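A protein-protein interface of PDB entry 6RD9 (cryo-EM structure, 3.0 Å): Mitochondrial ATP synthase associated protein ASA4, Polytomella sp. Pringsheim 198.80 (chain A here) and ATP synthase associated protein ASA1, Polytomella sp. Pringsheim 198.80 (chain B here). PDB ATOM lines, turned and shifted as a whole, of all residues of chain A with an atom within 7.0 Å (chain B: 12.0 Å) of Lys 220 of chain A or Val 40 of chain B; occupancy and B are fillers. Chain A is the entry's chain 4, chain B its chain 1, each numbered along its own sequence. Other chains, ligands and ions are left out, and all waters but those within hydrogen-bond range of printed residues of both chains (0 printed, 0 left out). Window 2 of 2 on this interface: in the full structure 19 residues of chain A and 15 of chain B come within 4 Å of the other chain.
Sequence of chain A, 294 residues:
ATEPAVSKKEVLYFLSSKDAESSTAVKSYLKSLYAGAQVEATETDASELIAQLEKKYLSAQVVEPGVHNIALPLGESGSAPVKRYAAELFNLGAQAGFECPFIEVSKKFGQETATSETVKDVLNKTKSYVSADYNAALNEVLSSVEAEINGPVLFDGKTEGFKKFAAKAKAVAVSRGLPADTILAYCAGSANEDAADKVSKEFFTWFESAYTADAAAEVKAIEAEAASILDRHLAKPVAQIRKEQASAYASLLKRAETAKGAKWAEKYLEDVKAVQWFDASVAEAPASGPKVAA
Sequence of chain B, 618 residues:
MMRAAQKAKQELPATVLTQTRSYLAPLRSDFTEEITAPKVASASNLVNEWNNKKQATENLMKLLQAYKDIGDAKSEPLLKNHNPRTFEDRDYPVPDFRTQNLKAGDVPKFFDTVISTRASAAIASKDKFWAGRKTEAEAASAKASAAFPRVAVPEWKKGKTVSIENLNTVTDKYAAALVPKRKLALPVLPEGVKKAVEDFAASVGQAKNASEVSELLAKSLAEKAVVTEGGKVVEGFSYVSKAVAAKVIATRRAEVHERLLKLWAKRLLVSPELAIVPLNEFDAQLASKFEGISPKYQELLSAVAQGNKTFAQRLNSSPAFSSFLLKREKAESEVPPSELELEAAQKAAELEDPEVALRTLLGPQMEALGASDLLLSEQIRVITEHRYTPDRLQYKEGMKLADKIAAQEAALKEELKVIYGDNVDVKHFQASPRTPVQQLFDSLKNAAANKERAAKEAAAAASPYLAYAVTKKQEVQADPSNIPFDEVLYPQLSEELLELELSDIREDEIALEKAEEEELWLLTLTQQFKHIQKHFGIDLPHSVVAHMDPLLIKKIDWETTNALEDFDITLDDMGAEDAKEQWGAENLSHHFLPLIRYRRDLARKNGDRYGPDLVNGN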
ATOM      1  N   LEU A  74     -19.942  -7.712  10.544  1.00  0.00           N
ATOM      2  CA  LEU A  74     -20.838  -8.817  10.822  1.00  0.00           C
ATOM      3  C   LEU A  74     -20.502  -9.993   9.932  1.00  0.00           C
ATOM      4  O   LEU A  74     -20.324  -9.834   8.723  1.00  0.00           O
ATOM      5  CB  LEU A  74     -22.277  -8.392  10.599  1.00  0.00           C
ATOM      6  CG  LEU A  74     -22.748  -7.228  11.421  1.00  0.00           C
ATOM      7  CD1 LEU A  74     -24.133  -6.906  11.073  1.00  0.00           C
ATOM      8  CD2 LEU A  74     -22.695  -7.641  12.827  1.00  0.00           C
ATOM      9  N   GLY A  75     -20.412 -11.172  10.529  1.00  0.00           N
ATOM     10  CA  GLY A  75     -20.152 -12.368   9.765  1.00  0.00           C
ATOM     11  C   GLY A  75     -18.773 -12.466   9.177  1.00  0.00           C
ATOM     12  O   GLY A  75     -18.576 -13.214   8.223  1.00  0.00           O
ATOM     13  N   GLU A  76     -17.810 -11.728   9.707  1.00  0.00           N
ATOM     14  CA  GLU A  76     -16.432 -11.795   9.253  1.00  0.00           C
ATOM     15  C   GLU A  76     -15.665 -12.765  10.129  1.00  0.00           C
ATOM     16  O   GLU A  76     -16.036 -13.021  11.275  1.00  0.00           O
ATOM     17  CB  GLU A  76     -15.750 -10.433   9.321  1.00  0.00           C
ATOM     18  CG  GLU A  76     -16.506  -9.309   8.691  1.00  0.00           C
ATOM     19  CD  GLU A  76     -16.194  -9.120   7.242  1.00  0.00           C
ATOM     20  OE1 GLU A  76     -15.065  -9.446   6.837  1.00  0.00           O
ATOM     21  OE2 GLU A  76     -17.081  -8.642   6.510  1.00  0.00           O
ATOM     22  N   ALA A 215     -15.792  -5.148  21.290  1.00  0.00           N
ATOM     23  CA  ALA A 215     -16.320  -4.980  19.950  1.00  0.00           C
ATOM     24  C   ALA A 215     -16.843  -6.293  19.415  1.00  0.00           C
ATOM     25  O   ALA A 215     -17.907  -6.329  18.798  1.00  0.00           O
ATOM     26  CB  ALA A 215     -15.250  -4.420  19.030  1.00  0.00           C
ATOM     27  N   ALA A 216     -16.134  -7.389  19.668  1.00  0.00           N
ATOM     28  CA  ALA A 216     -16.578  -8.678  19.164  1.00  0.00           C
ATOM     29  C   ALA A 216     -17.795  -9.179  19.905  1.00  0.00           C
ATOM     30  O   ALA A 216     -18.552  -9.974  19.360  1.00  0.00           O
ATOM     31  CB  ALA A 216     -15.463  -9.707  19.251  1.00  0.00           C
ATOM     32  N   ALA A 217     -18.001  -8.745  21.137  1.00  0.00           N
ATOM     33  CA  ALA A 217     -19.244  -9.063  21.818  1.00  0.00           C
ATOM     34  C   ALA A 217     -20.383  -8.194  21.342  1.00  0.00           C
ATOM     35  O   ALA A 217     -21.541  -8.551  21.547  1.00  0.00           O
ATOM     36  CB  ALA A 217     -19.088  -8.900  23.318  1.00  0.00           C
ATOM     37  N   GLU A 218     -20.083  -7.044  20.756  1.00  0.00           N
ATOM     38  CA  GLU A 218     -21.112  -6.194  20.184  1.00  0.00           C
ATOM     39  C   GLU A 218     -21.524  -6.682  18.814  1.00  0.00           C
ATOM     40  O   GLU A 218     -22.687  -6.564  18.439  1.00  0.00           O
ATOM     41  CB  GLU A 218     -20.601  -4.761  20.101  1.00  0.00           C
ATOM     42  CG  GLU A 218     -21.636  -3.761  19.717  1.00  0.00           C
ATOM     43  CD  GLU A 218     -22.715  -3.624  20.757  1.00  0.00           C
ATOM     44  OE1 GLU A 218     -22.392  -3.178  21.879  1.00  0.00           O
ATOM     45  OE2 GLU A 218     -23.882  -3.969  20.456  1.00  0.00           O
ATOM     46  N   VAL A 219     -20.577  -7.223  18.059  1.00  0.00           N
ATOM     47  CA  VAL A 219     -20.865  -7.811  16.763  1.00  0.00           C
ATOM     48  C   VAL A 219     -21.641  -9.101  16.927  1.00  0.00           C
ATOM     49  O   VAL A 219     -22.614  -9.342  16.217  1.00  0.00           O
ATOM     50  CB  VAL A 219     -19.545  -8.023  16.013  1.00  0.00           C
ATOM     51  CG1 VAL A 219     -19.733  -8.848  14.796  1.00  0.00           C
ATOM     52  CG2 VAL A 219     -18.965  -6.709  15.673  1.00  0.00           C
ATOM     53  N   LYS A 220     -21.274  -9.924  17.906  1.00  0.00           N
ATOM     54  CA  LYS A 220     -21.982 -11.176  18.134  1.00  0.00           C
ATOM     55  C   LYS A 220     -23.371 -10.977  18.703  1.00  0.00           C
ATOM     56  O   LYS A 220     -24.125 -11.942  18.779  1.00  0.00           O
ATOM     57  CB  LYS A 220     -21.198 -12.080  19.073  1.00  0.00           C
ATOM     58  CG  LYS A 220     -19.997 -12.724  18.444  1.00  0.00           C
ATOM     59  CD  LYS A 220     -20.362 -13.529  17.221  1.00  0.00           C
ATOM     60  CE  LYS A 220     -19.118 -13.953  16.466  1.00  0.00           C
ATOM     61  NZ  LYS A 220     -19.428 -14.894  15.363  1.00  0.00           N
ATOM     62  N   ALA A 221     -23.723  -9.778  19.126  1.00  0.00           N
ATOM     63  CA  ALA A 221     -25.089  -9.508  19.522  1.00  0.00           C
ATOM     64  C   ALA A 221     -25.910  -8.911  18.407  1.00  0.00           C
ATOM     65  O   ALA A 221     -27.132  -9.030  18.427  1.00  0.00           O
ATOM     66  CB  ALA A 221     -25.119  -8.562  20.706  1.00  0.00           C
ATOM     67  N   ILE A 222     -25.273  -8.226  17.463  1.00  0.00           N
ATOM     68  CA  ILE A 222     -25.972  -7.749  16.279  1.00  0.00           C
ATOM     69  C   ILE A 222     -26.193  -8.897  15.316  1.00  0.00           C
ATOM     70  O   ILE A 222     -27.230  -8.984  14.659  1.00  0.00           O
ATOM     71  CB  ILE A 222     -25.182  -6.597  15.634  1.00  0.00           C
ATOM     72  CG1 ILE A 222     -25.133  -5.407  16.566  1.00  0.00           C
ATOM     73  CG2 ILE A 222     -25.803  -6.143  14.368  1.00  0.00           C
ATOM     74  CD1 ILE A 222     -26.475  -4.902  16.952  1.00  0.00           C
ATOM     75  N   GLU A 223     -25.234  -9.811  15.240  1.00  0.00           N
ATOM     76  CA  GLU A 223     -25.399 -11.017  14.449  1.00  0.00           C
ATOM     77  C   GLU A 223     -26.512 -11.887  14.991  1.00  0.00           C
ATOM     78  O   GLU A 223     -27.252 -12.504  14.228  1.00  0.00           O
ATOM     79  CB  GLU A 223     -24.108 -11.810  14.446  1.00  0.00           C
ATOM     80  CG  GLU A 223     -23.044 -11.260  13.590  1.00  0.00           C
ATOM     81  CD  GLU A 223     -21.848 -12.144  13.587  1.00  0.00           C
ATOM     82  OE1 GLU A 223     -21.947 -13.245  14.143  1.00  0.00           O
ATOM     83  OE2 GLU A 223     -20.809 -11.757  13.033  1.00  0.00           O
ATOM     84  N   ALA A 224     -26.633 -11.966  16.304  1.00  0.00           N
ATOM     85  CA  ALA A 224     -27.672 -12.777  16.907  1.00  0.00           C
ATOM     86  C   ALA A 224     -29.020 -12.092  16.878  1.00  0.00           C
ATOM     87  O   ALA A 224     -30.044 -12.768  16.886  1.00  0.00           O
ATOM     88  CB  ALA A 224     -27.294 -13.115  18.337  1.00  0.00           C
ATOM     89  N   GLU A 225     -29.052 -10.767  16.881  1.00  0.00           N
ATOM     90  CA  GLU A 225     -30.316 -10.062  16.745  1.00  0.00           C
ATOM     91  C   GLU A 225     -30.823 -10.137  15.322  1.00  0.00           C
ATOM     92  O   GLU A 225     -32.016 -10.338  15.096  1.00  0.00           O
ATOM     93  CB  GLU A 225     -30.157  -8.607  17.166  1.00  0.00           C
ATOM     94  CG  GLU A 225     -31.330  -7.738  16.816  1.00  0.00           C
ATOM     95  CD  GLU A 225     -31.252  -6.360  17.411  1.00  0.00           C
ATOM     96  OE1 GLU A 225     -32.303  -5.696  17.509  1.00  0.00           O
ATOM     97  OE2 GLU A 225     -30.143  -5.936  17.785  1.00  0.00           O
ATOM     98  N   THR B  36     -23.080  -2.350  29.946  1.00  0.00           N
ATOM     99  CA  THR B  36     -23.532  -3.716  30.105  1.00  0.00           C
ATOM    100  C   THR B  36     -23.031  -4.579  28.964  1.00  0.00           C
ATOM    101  O   THR B  36     -22.401  -4.108  28.020  1.00  0.00           O
ATOM    102  CB  THR B  36     -25.056  -3.783  30.173  1.00  0.00           C
ATOM    103  OG1 THR B  36     -25.608  -3.048  29.079  1.00  0.00           O
ATOM    104  CG2 THR B  36     -25.567  -3.234  31.475  1.00  0.00           C
ATOM    105  N   ALA B  37     -23.289  -5.869  29.098  1.00  0.00           N
ATOM    106  CA  ALA B  37     -23.076  -6.798  28.014  1.00  0.00           C
ATOM    107  C   ALA B  37     -24.210  -6.648  27.003  1.00  0.00           C
ATOM    108  O   ALA B  37     -25.324  -6.275  27.371  1.00  0.00           O
ATOM    109  CB  ALA B  37     -23.015  -8.221  28.556  1.00  0.00           C
ATOM    110  N   PRO B  38     -23.956  -6.915  25.724  1.00  0.00           N
ATOM    111  CA  PRO B  38     -24.916  -6.499  24.700  1.00  0.00           C
ATOM    112  C   PRO B  38     -26.099  -7.416  24.414  1.00  0.00           C
ATOM    113  O   PRO B  38     -26.722  -7.218  23.367  1.00  0.00           O
ATOM    114  CB  PRO B  38     -24.038  -6.373  23.455  1.00  0.00           C
ATOM    115  CG  PRO B  38     -22.669  -6.415  23.919  1.00  0.00           C
ATOM    116  CD  PRO B  38     -22.664  -7.245  25.112  1.00  0.00           C
ATOM    117  N   LYS B  39     -26.422  -8.385  25.280  1.00  0.00           N
ATOM    118  CA  LYS B  39     -27.652  -9.197  25.222  1.00  0.00           C
ATOM    119  C   LYS B  39     -27.760 -10.021  23.931  1.00  0.00           C
ATOM    120  O   LYS B  39     -28.578  -9.745  23.057  1.00  0.00           O
ATOM    121  CB  LYS B  39     -28.906  -8.333  25.387  1.00  0.00           C
ATOM    122  CG  LYS B  39     -29.187  -7.897  26.792  1.00  0.00           C
ATOM    123  CD  LYS B  39     -29.606  -9.056  27.662  1.00  0.00           C
ATOM    124  CE  LYS B  39     -29.735  -8.627  29.108  1.00  0.00           C
ATOM    125  NZ  LYS B  39     -28.432  -8.180  29.672  1.00  0.00           N
ATOM    126  N   VAL B  40     -26.900 -11.036  23.833  1.00  0.00           N
ATOM    127  CA  VAL B  40     -26.945 -11.979  22.716  1.00  0.00           C
ATOM    128  C   VAL B  40     -28.259 -12.746  22.733  1.00  0.00           C
ATOM    129  O   VAL B  40     -28.577 -13.432  23.708  1.00  0.00           O
ATOM    130  CB  VAL B  40     -25.763 -12.941  22.782  1.00  0.00           C
ATOM    131  CG1 VAL B  40     -25.856 -13.959  21.691  1.00  0.00           C
ATOM    132  CG2 VAL B  40     -24.472 -12.197  22.670  1.00  0.00           C
ATOM    133  N   ALA B  41     -29.026 -12.639  21.650  1.00  0.00           N
ATOM    134  CA  ALA B  41     -30.295 -13.343  21.548  1.00  0.00           C
ATOM    135  C   ALA B  41     -30.070 -14.816  21.252  1.00  0.00           C
ATOM    136  O   ALA B  41     -28.970 -15.253  20.916  1.00  0.00           O
ATOM    137  CB  ALA B  41     -31.176 -12.737  20.463  1.00  0.00           C
ATOM    138  N   SER B  42     -31.139 -15.584  21.375  1.00  0.00           N
ATOM    139  CA  SER B  42     -31.058 -17.031  21.303  1.00  0.00           C
ATOM    140  C   SER B  42     -31.120 -17.511  19.864  1.00  0.00           C
ATOM    141  O   SER B  42     -31.630 -16.826  18.976  1.00  0.00           O
ATOM    142  CB  SER B  42     -32.187 -17.658  22.109  1.00  0.00           C
ATOM    143  OG  SER B  42     -33.394 -16.957  21.873  1.00  0.00           O
ATOM    144  N   ALA B  43     -30.595 -18.710  19.646  1.00  0.00           N
ATOM    145  CA  ALA B  43     -30.608 -19.310  18.322  1.00  0.00           C
ATOM    146  C   ALA B  43     -32.030 -19.687  17.953  1.00  0.00           C
ATOM    147  O   ALA B  43     -32.634 -20.554  18.591  1.00  0.00           O
ATOM    148  CB  ALA B  43     -29.707 -20.535  18.284  1.00  0.00           C
ATOM    149  N   SER B  44     -32.574 -19.015  16.948  1.00  0.00           N
ATOM    150  CA  SER B  44     -33.931 -19.291  16.520  1.00  0.00           C
ATOM    151  C   SER B  44     -33.977 -20.627  15.804  1.00  0.00           C
ATOM    152  O   SER B  44     -33.040 -21.012  15.106  1.00  0.00           O
ATOM    153  CB  SER B  44     -34.433 -18.179  15.609  1.00  0.00           C
ATOM    154  OG  SER B  44     -35.840 -18.211  15.493  1.00  0.00           O
ATOM    155  N   LYS B 158     -22.450 -17.189  -2.061  1.00  0.00           N
ATOM    156  CA  LYS B 158     -22.625 -16.441  -0.817  1.00  0.00           C
ATOM    157  C   LYS B 158     -22.559 -14.938  -1.041  1.00  0.00           C
ATOM    158  O   LYS B 158     -23.473 -14.201  -0.660  1.00  0.00           O
ATOM    159  CB  LYS B 158     -21.583 -16.875   0.204  1.00  0.00           C
ATOM    160  CG  LYS B 158     -21.758 -16.247   1.564  1.00  0.00           C
ATOM    161  CD  LYS B 158     -23.042 -16.665   2.194  1.00  0.00           C
ATOM    162  CE  LYS B 158     -22.912 -16.787   3.684  1.00  0.00           C
ATOM    163  NZ  LYS B 158     -21.919 -17.793   4.093  1.00  0.00           N
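OE1 of Glu 223 of chain A is in salt-bridge range of NZ of Lys 220 of chain A, at 3.2 Å.
Pro 38 of chain B touches Ala 217 of chain A.
CG of Pro 38 of chain B touches OE1 of Glu 218 of chain A (3.8 Å).
Val 40 of chain B touches Lys 220 of chain A.
Pro 38 of chain B touches Ala 221 of chain A.
Ala 224 of chain A touches Val 40 of chain B.
O of Ala 41 of chain B touches CB of Ala 224 of chain A, at 3.7 Å.
No residue of chain B comes within 4 Å of Ala 216 of chain A.
Ala 217 of chain A touches just one residue of chain B: Pro 38 (3.4 Å).
No residue of chain B comes within 4 Å of Val 219 of chain A.
Of chain B, only Val 40 (3.9 Å) comes within 4 Å of Lys 220 of chain A.
Ala 221 of chain A touches just one residue of chain B: Pro 38 (3.4 Å).
No residue of chain B comes within 4 Å of Glu 223 of chain A.
Printed residues of chain A within 4 Å of Pro 38 of chain B: Ala 217, Glu 218 and Ala 221.
Val 40 of chain B touches just these residues of chain A: Lys 220 and Ala 224.
Of the printed residues of chain A, Ala 41 of chain B touches Ala 224.
Ser 44 of chain B touches none of the printed residues of chain A.
The nearest residue of chain A that does not touch Val 40 of chain B is Ala 221 of chain A (4.2 Å).
The nearest printed residue of chain A that does not touch Ala 41 of chain B is Glu 225 of chain A (4.6 Å).
Printed residues of chain A that touch a printed residue of chain B: Ala 217, Glu 218, Lys 220, Ala 221 and Ala 224.
Hydrophobic or aromatic side chains of chain A within 4 Å of the printed part of chain B: Ala 221 and Ala 224.
Among the printed residues, 6 pairs touch across the chains.
Among the printed residues, no Asp or Glu carboxylate lies within 4 Å of a Lys or Arg side-chain nitrogen of the other chain.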
